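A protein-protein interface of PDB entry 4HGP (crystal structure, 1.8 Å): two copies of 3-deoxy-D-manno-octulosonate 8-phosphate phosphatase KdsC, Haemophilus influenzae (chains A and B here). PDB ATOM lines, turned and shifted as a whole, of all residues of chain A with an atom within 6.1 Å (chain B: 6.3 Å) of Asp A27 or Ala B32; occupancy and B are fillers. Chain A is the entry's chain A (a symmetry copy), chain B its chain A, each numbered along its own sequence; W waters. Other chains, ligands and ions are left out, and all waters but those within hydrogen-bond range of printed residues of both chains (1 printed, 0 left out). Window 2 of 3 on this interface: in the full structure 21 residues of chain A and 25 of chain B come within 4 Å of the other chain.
N of Tyr A26 sits at hydrogen-bond distance from O of Lys B34, 2.8 Å away.
The guanidinium group (NH1) of Arg B67 lies within hydrogen-bond range of the backbone carbonyl oxygen (O) of Asn A29.
NH1 of Arg B68 is in hydrogen-bond range of OH of Tyr A26 (3.0 Å).
Printed residues of chain B that touch a printed residue of chain A: Ala B32, Ile B33, Lys B34, Ile B64, Arg B67 and Arg B68.
Hydrophobic or aromatic side chains of chain B within 4 Å of the printed part of chain A: Ile B33 and Ile B64.
Hydrophobic or aromatic side chains of chain A that line the printed part of chain B: His A25 and Tyr A26.
Among the printed residues, no Asp or Glu carboxylate lies within 4 Å of a Lys or Arg side-chain nitrogen of the other chain.
Asp A27 touches Ala B32, but with the chains exchanged Ala A32 does not touch Asp B27 (9.9 Å).
Positions printed for both chains: 25, 26, 27, 28, 30, 31 and 32.
Asp A27 touches two residues of chain B.
Of chain A, only Asp A27 (3.7 Å) comes within 4 Å of Ala B32.
Of the printed residues of chain B, Gly A30 touches Arg B67.
Of the printed residues of chain B, Tyr A26 touches Ile B33, Lys B34, Ile B64 and Arg B68.
Printed residues of chain B within 4 Å of Asn A29: Arg B67.
Printed residues of chain A within 4 Å of Ile B64: Tyr A26 (3.3 Å), Asp A27 (3.6 Å) and Ala A28 (3.95 Å).
Printed residues of chain B within 4 Å of Ala A28: Ile B64 and Arg B67.
The nearest residue of chain B that does not touch Asp A27 is Arg B67 (4.1 Å).
O of His B25 is in hydrogen-bond range of N of Ala B32, at 2.8 Å.
The backbone carbonyl oxygen of His B25 sits at hydrogen-bond distance from the backbone NH of Ile B33 (3.4 Å).
OE1 of Glu B31 is in salt-bridge range of NZ of Lys B34.
The backbone carbonyl oxygen (O) of His A25 is in hydrogen-bond range of the backbone NH (N) of Ala A32, 2.8 Å away.
The backbone NH (N) of Asn A29 is in hydrogen-bond range of the side-chain carboxylate (OD1) of Asp A27, 2.9 Å away.
Among the printed residues, pairs that only touch across the chains: His A25 with Ile B33, His A25 with Lys B34, Tyr A26 with Ile B33, Tyr A26 with Ile B64, Asp A27 with Ala B32, Asp A27 with Ile B64, Ala A28 with Ile B64, Ala A28 with Arg B67 and Gly A30 with Arg B67.
Water W1 lies within hydrogen-bond range of NH1 of Arg B67 (2.5 Å) and O of Ala A28 (3.5 Å).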
ATOM      1  N   HIS A  25     -12.636  12.321 -21.863  1.00  0.00           N
ATOM      2  CA  HIS A  25     -12.028  13.195 -22.853  1.00  0.00           C
ATOM      3  C   HIS A  25     -12.894  13.226 -24.094  1.00  0.00           C
ATOM      4  O   HIS A  25     -12.790  12.358 -24.954  1.00  0.00           O
ATOM      5  CB  HIS A  25     -10.609  12.732 -23.211  1.00  0.00           C
ATOM      6  CG  HIS A  25      -9.704  12.569 -22.028  1.00  0.00           C
ATOM      7  ND1 HIS A  25      -9.572  13.528 -21.047  1.00  0.00           N
ATOM      8  CD2 HIS A  25      -8.882  11.555 -21.675  1.00  0.00           C
ATOM      9  CE1 HIS A  25      -8.711  13.108 -20.139  1.00  0.00           C
ATOM     10  NE2 HIS A  25      -8.279  11.915 -20.494  1.00  0.00           N
ATOM     11  N   TYR A  26     -13.749  14.235 -24.178  1.00  0.00           N
ATOM     12  CA  TYR A  26     -14.691  14.363 -25.278  1.00  0.00           C
ATOM     13  C   TYR A  26     -14.080  14.988 -26.529  1.00  0.00           C
ATOM     14  O   TYR A  26     -13.211  15.856 -26.446  1.00  0.00           O
ATOM     15  CB  TYR A  26     -15.872  15.233 -24.832  1.00  0.00           C
ATOM     16  CG  TYR A  26     -17.017  14.469 -24.215  1.00  0.00           C
ATOM     17  CD1 TYR A  26     -16.887  13.860 -22.976  1.00  0.00           C
ATOM     18  CD2 TYR A  26     -18.240  14.363 -24.873  1.00  0.00           C
ATOM     19  CE1 TYR A  26     -17.938  13.158 -22.415  1.00  0.00           C
ATOM     20  CE2 TYR A  26     -19.292  13.670 -24.322  1.00  0.00           C
ATOM     21  CZ  TYR A  26     -19.138  13.069 -23.090  1.00  0.00           C
ATOM     22  OH  TYR A  26     -20.188  12.376 -22.535  1.00  0.00           O
ATOM     23  N   ASP A  27     -14.542  14.553 -27.697  1.00  0.00           N
ATOM     24  CA  ASP A  27     -14.496  15.439 -28.854  1.00  0.00           C
ATOM     25  C   ASP A  27     -15.928  15.729 -29.304  1.00  0.00           C
ATOM     26  O   ASP A  27     -16.861  15.628 -28.513  1.00  0.00           O
ATOM     27  CB  ASP A  27     -13.587  14.934 -29.987  1.00  0.00           C
ATOM     28  CG  ASP A  27     -14.030  13.605 -30.581  1.00  0.00           C
ATOM     29  OD1 ASP A  27     -15.175  13.175 -30.370  1.00  0.00           O
ATOM     30  OD2 ASP A  27     -13.209  12.989 -31.296  1.00  0.00           O
ATOM     31  N   ALA A  28     -16.099  16.104 -30.560  1.00  0.00           N
ATOM     32  CA  ALA A  28     -17.421  16.472 -31.050  1.00  0.00           C
ATOM     33  C   ALA A  28     -18.386  15.285 -31.056  1.00  0.00           C
ATOM     34  O   ALA A  28     -19.597  15.461 -31.001  1.00  0.00           O
ATOM     35  CB  ALA A  28     -17.313  17.069 -32.437  1.00  0.00           C
ATOM     36  N   ASN A  29     -17.843  14.074 -31.114  1.00  0.00           N
ATOM     37  CA  ASN A  29     -18.671  12.888 -31.253  1.00  0.00           C
ATOM     38  C   ASN A  29     -18.842  12.078 -29.970  1.00  0.00           C
ATOM     39  O   ASN A  29     -19.422  10.992 -29.985  1.00  0.00           O
ATOM     40  CB  ASN A  29     -18.140  12.010 -32.388  1.00  0.00           C
ATOM     41  CG  ASN A  29     -18.295  12.663 -33.757  1.00  0.00           C
ATOM     42  OD1 ASN A  29     -17.335  12.776 -34.515  1.00  0.00           O
ATOM     43  ND2 ASN A  29     -19.511  13.089 -34.078  1.00  0.00           N
ATOM     44  N   GLY A  30     -18.353  12.625 -28.862  1.00  0.00           N
ATOM     45  CA  GLY A  30     -18.442  11.973 -27.566  1.00  0.00           C
ATOM     46  C   GLY A  30     -17.055  11.647 -27.047  1.00  0.00           C
ATOM     47  O   GLY A  30     -16.109  12.387 -27.320  1.00  0.00           O
ATOM     48  N   GLU A  31     -16.936  10.545 -26.308  1.00  0.00           N
ATOM     49  CA  GLU A  31     -15.637  10.059 -25.832  1.00  0.00           C
ATOM     50  C   GLU A  31     -14.676   9.803 -26.979  1.00  0.00           C
ATOM     51  O   GLU A  31     -14.995   9.056 -27.912  1.00  0.00           O
ATOM     52  CB  GLU A  31     -15.798   8.770 -25.027  1.00  0.00           C
ATOM     53  CG  GLU A  31     -16.283   8.968 -23.613  1.00  0.00           C
ATOM     54  CD  GLU A  31     -16.063   7.735 -22.775  1.00  0.00           C
ATOM     55  OE1 GLU A  31     -14.968   7.594 -22.195  1.00  0.00           O
ATOM     56  OE2 GLU A  31     -16.983   6.901 -22.695  1.00  0.00           O
ATOM     57  N   ALA A  32     -13.495  10.411 -26.885  1.00  0.00           N
ATOM     58  CA  ALA A  32     -12.512  10.401 -27.966  1.00  0.00           C
ATOM     59  C   ALA A  32     -11.212   9.729 -27.545  1.00  0.00           C
ATOM     60  O   ALA A  32     -10.531   9.116 -28.361  1.00  0.00           O
ATOM     61  CB  ALA A  32     -12.233  11.802 -28.412  1.00  0.00           C
ATOM     62  N   HIS B  25      -7.185  21.865 -24.574  1.00  0.00           N
ATOM     63  CA  HIS B  25      -6.386  20.946 -25.368  1.00  0.00           C
ATOM     64  C   HIS B  25      -6.540  21.286 -26.835  1.00  0.00           C
ATOM     65  O   HIS B  25      -7.487  20.853 -27.484  1.00  0.00           O
ATOM     66  CB  HIS B  25      -6.796  19.489 -25.118  1.00  0.00           C
ATOM     67  CG  HIS B  25      -6.776  19.089 -23.675  1.00  0.00           C
ATOM     68  ND1 HIS B  25      -5.712  19.349 -22.839  1.00  0.00           N
ATOM     69  CD2 HIS B  25      -7.694  18.440 -22.922  1.00  0.00           C
ATOM     70  CE1 HIS B  25      -5.979  18.882 -21.633  1.00  0.00           C
ATOM     71  NE2 HIS B  25      -7.175  18.329 -21.655  1.00  0.00           N
ATOM     72  N   TYR B  26      -5.600  22.065 -27.351  1.00  0.00           N
ATOM     73  CA  TYR B  26      -5.648  22.530 -28.728  1.00  0.00           C
ATOM     74  C   TYR B  26      -5.124  21.506 -29.731  1.00  0.00           C
ATOM     75  O   TYR B  26      -4.201  20.747 -29.439  1.00  0.00           O
ATOM     76  CB  TYR B  26      -4.810  23.807 -28.859  1.00  0.00           C
ATOM     77  CG  TYR B  26      -5.572  25.086 -28.620  1.00  0.00           C
ATOM     78  CD1 TYR B  26      -6.037  25.418 -27.356  1.00  0.00           C
ATOM     79  CD2 TYR B  26      -5.823  25.972 -29.664  1.00  0.00           C
ATOM     80  CE1 TYR B  26      -6.738  26.590 -27.141  1.00  0.00           C
ATOM     81  CE2 TYR B  26      -6.517  27.142 -29.460  1.00  0.00           C
ATOM     82  CZ  TYR B  26      -6.972  27.449 -28.195  1.00  0.00           C
ATOM     83  OH  TYR B  26      -7.665  28.619 -27.987  1.00  0.00           O
ATOM     84  N   ASP B  27      -5.708  21.491 -30.925  1.00  0.00           N
ATOM     85  CA  ASP B  27      -4.950  21.031 -32.082  1.00  0.00           C
ATOM     86  C   ASP B  27      -4.798  22.196 -33.061  1.00  0.00           C
ATOM     87  O   ASP B  27      -4.871  23.355 -32.664  1.00  0.00           O
ATOM     88  CB  ASP B  27      -5.516  19.756 -32.730  1.00  0.00           C
ATOM     89  CG  ASP B  27      -6.925  19.923 -33.278  1.00  0.00           C
ATOM     90  OD1 ASP B  27      -7.399  21.055 -33.453  1.00  0.00           O
ATOM     91  OD2 ASP B  27      -7.562  18.883 -33.558  1.00  0.00           O
ATOM     92  N   ALA B  28      -4.570  21.892 -34.326  1.00  0.00           N
ATOM     93  CA  ALA B  28      -4.338  22.941 -35.310  1.00  0.00           C
ATOM     94  C   ALA B  28      -5.576  23.814 -35.527  1.00  0.00           C
ATOM     95  O   ALA B  28      -5.470  24.960 -35.945  1.00  0.00           O
ATOM     96  CB  ALA B  28      -3.887  22.333 -36.621  1.00  0.00           C
ATOM     97  N   GLY B  30      -7.979  24.557 -33.170  1.00  0.00           N
ATOM     98  CA  GLY B  30      -8.494  25.112 -31.929  1.00  0.00           C
ATOM     99  C   GLY B  30      -8.678  24.015 -30.900  1.00  0.00           C
ATOM    100  O   GLY B  30      -7.914  23.048 -30.892  1.00  0.00           O
ATOM    101  N   GLU B  31      -9.685  24.161 -30.040  1.00  0.00           N
ATOM    102  CA  GLU B  31     -10.037  23.126 -29.063  1.00  0.00           C
ATOM    103  C   GLU B  31     -10.354  21.802 -29.734  1.00  0.00           C
ATOM    104  O   GLU B  31     -11.215  21.736 -30.621  1.00  0.00           O
ATOM    105  CB  GLU B  31     -11.240  23.554 -28.224  1.00  0.00           C
ATOM    106  CG  GLU B  31     -10.922  24.536 -27.125  1.00  0.00           C
ATOM    107  CD  GLU B  31     -12.044  24.623 -26.120  1.00  0.00           C
ATOM    108  OE1 GLU B  31     -12.054  23.822 -25.165  1.00  0.00           O
ATOM    109  OE2 GLU B  31     -12.919  25.492 -26.285  1.00  0.00           O
ATOM    110  N   ALA B  32      -9.668  20.752 -29.285  1.00  0.00           N
ATOM    111  CA  ALA B  32      -9.733  19.436 -29.918  1.00  0.00           C
ATOM    112  C   ALA B  32     -10.275  18.377 -28.969  1.00  0.00           C
ATOM    113  O   ALA B  32     -10.929  17.429 -29.395  1.00  0.00           O
ATOM    114  CB  ALA B  32      -8.373  19.035 -30.397  1.00  0.00           C
ATOM    115  N   ILE B  33      -9.979  18.539 -27.683  1.00  0.00           N
ATOM    116  CA  ILE B  33     -10.509  17.671 -26.635  1.00  0.00           C
ATOM    117  C   ILE B  33     -10.898  18.519 -25.429  1.00  0.00           C
ATOM    118  O   ILE B  33     -10.202  19.477 -25.102  1.00  0.00           O
ATOM    119  CB  ILE B  33      -9.487  16.562 -26.232  1.00  0.00           C
ATOM    120  CG1 ILE B  33      -9.395  15.515 -27.348  1.00  0.00           C
ATOM    121  CG2 ILE B  33      -9.901  15.882 -24.948  1.00  0.00           C
ATOM    122  CD1 ILE B  33      -8.499  14.333 -27.029  1.00  0.00           C
ATOM    123  N   LYS B  34     -12.044  18.211 -24.818  1.00  0.00           N
ATOM    124  CA  LYS B  34     -12.377  18.756 -23.498  1.00  0.00           C
ATOM    125  C   LYS B  34     -12.498  17.590 -22.533  1.00  0.00           C
ATOM    126  O   LYS B  34     -13.107  16.572 -22.862  1.00  0.00           O
ATOM    127  CB  LYS B  34     -13.684  19.563 -23.499  1.00  0.00           C
ATOM    128  CG  LYS B  34     -13.739  20.735 -24.449  1.00  0.00           C
ATOM    129  CD  LYS B  34     -14.985  21.566 -24.207  1.00  0.00           C
ATOM    130  CE  LYS B  34     -14.900  22.351 -22.907  1.00  0.00           C
ATOM    131  NZ  LYS B  34     -13.704  23.244 -22.815  1.00  0.00           N
ATOM    132  N   PRO B  63     -18.205  22.631 -30.419  1.00  0.00           N
ATOM    133  CA  PRO B  63     -19.039  21.449 -30.670  1.00  0.00           C
ATOM    134  C   PRO B  63     -18.812  20.361 -29.617  1.00  0.00           C
ATOM    135  O   PRO B  63     -19.733  19.597 -29.310  1.00  0.00           O
ATOM    136  CB  PRO B  63     -18.552  20.965 -32.038  1.00  0.00           C
ATOM    137  CG  PRO B  63     -17.961  22.168 -32.682  1.00  0.00           C
ATOM    138  CD  PRO B  63     -17.345  22.955 -31.569  1.00  0.00           C
ATOM    139  N   ILE B  64     -17.598  20.309 -29.074  1.00  0.00           N
ATOM    140  CA  ILE B  64     -17.252  19.366 -28.013  1.00  0.00           C
ATOM    141  C   ILE B  64     -18.073  19.608 -26.757  1.00  0.00           C
ATOM    142  O   ILE B  64     -18.630  18.677 -26.187  1.00  0.00           O
ATOM    143  CB  ILE B  64     -15.779  19.482 -27.612  1.00  0.00           C
ATOM    144  CG1 ILE B  64     -14.882  19.455 -28.848  1.00  0.00           C
ATOM    145  CG2 ILE B  64     -15.410  18.361 -26.638  1.00  0.00           C
ATOM    146  CD1 ILE B  64     -13.420  19.504 -28.524  1.00  0.00           C
ATOM    147  N   LEU B  65     -18.114  20.862 -26.312  1.00  0.00           N
ATOM    148  CA  LEU B  65     -18.891  21.219 -25.130  1.00  0.00           C
ATOM    149  C   LEU B  65     -20.377  20.982 -25.384  1.00  0.00           C
ATOM    150  O   LEU B  65     -21.082  20.424 -24.542  1.00  0.00           O
ATOM    151  CB  LEU B  65     -18.615  22.665 -24.711  1.00  0.00           C
ATOM    152  CG  LEU B  65     -19.518  23.291 -23.641  1.00  0.00           C
ATOM    153  CD1 LEU B  65     -19.610  22.412 -22.398  1.00  0.00           C
ATOM    154  CD2 LEU B  65     -19.026  24.674 -23.269  1.00  0.00           C
ATOM    155  N   ARG B  67     -21.645  18.783 -27.233  1.00  0.00           N
ATOM    156  CA  ARG B  67     -21.883  17.342 -27.190  1.00  0.00           C
ATOM    157  C   ARG B  67     -22.021  16.824 -25.749  1.00  0.00           C
ATOM    158  O   ARG B  67     -22.925  16.042 -25.445  1.00  0.00           O
ATOM    159  CB  ARG B  67     -20.762  16.603 -27.922  1.00  0.00           C
ATOM    160  CG  ARG B  67     -20.855  15.097 -27.838  1.00  0.00           C
ATOM    161  CD  ARG B  67     -22.216  14.604 -28.301  1.00  0.00           C
ATOM    162  NE  ARG B  67     -22.362  13.165 -28.118  1.00  0.00           N
ATOM    163  CZ  ARG B  67     -22.203  12.267 -29.083  1.00  0.00           C
ATOM    164  NH1 ARG B  67     -21.896  12.655 -30.309  1.00  0.00           N
ATOM    165  NH2 ARG B  67     -22.367  10.982 -28.825  1.00  0.00           N
ATOM    166  N   ARG B  68     -21.120  17.259 -24.868  1.00  0.00           N
ATOM    167  CA  ARG B  68     -21.182  16.884 -23.454  1.00  0.00           C
ATOM    168  C   ARG B  68     -22.490  17.372 -22.824  1.00  0.00           C
ATOM    169  O   ARG B  68     -23.124  16.667 -22.030  1.00  0.00           O
ATOM    170  CB  ARG B  68     -19.978  17.447 -22.698  1.00  0.00           C
ATOM    171  CG  ARG B  68     -19.969  17.128 -21.209  1.00  0.00           C
ATOM    172  CD  ARG B  68     -19.881  15.632 -20.937  1.00  0.00           C
ATOM    173  NE  ARG B  68     -19.628  15.355 -19.520  1.00  0.00           N
ATOM    174  CZ  ARG B  68     -19.874  14.192 -18.922  1.00  0.00           C
ATOM    175  NH1 ARG B  68     -20.379  13.185 -19.617  1.00  0.00           N
ATOM    176  NH2 ARG B  68     -19.621  14.041 -17.629  1.00  0.00           N
HETATM  177  O   HOH W   1     -22.796  14.432 -31.840  1.00  0.00           O
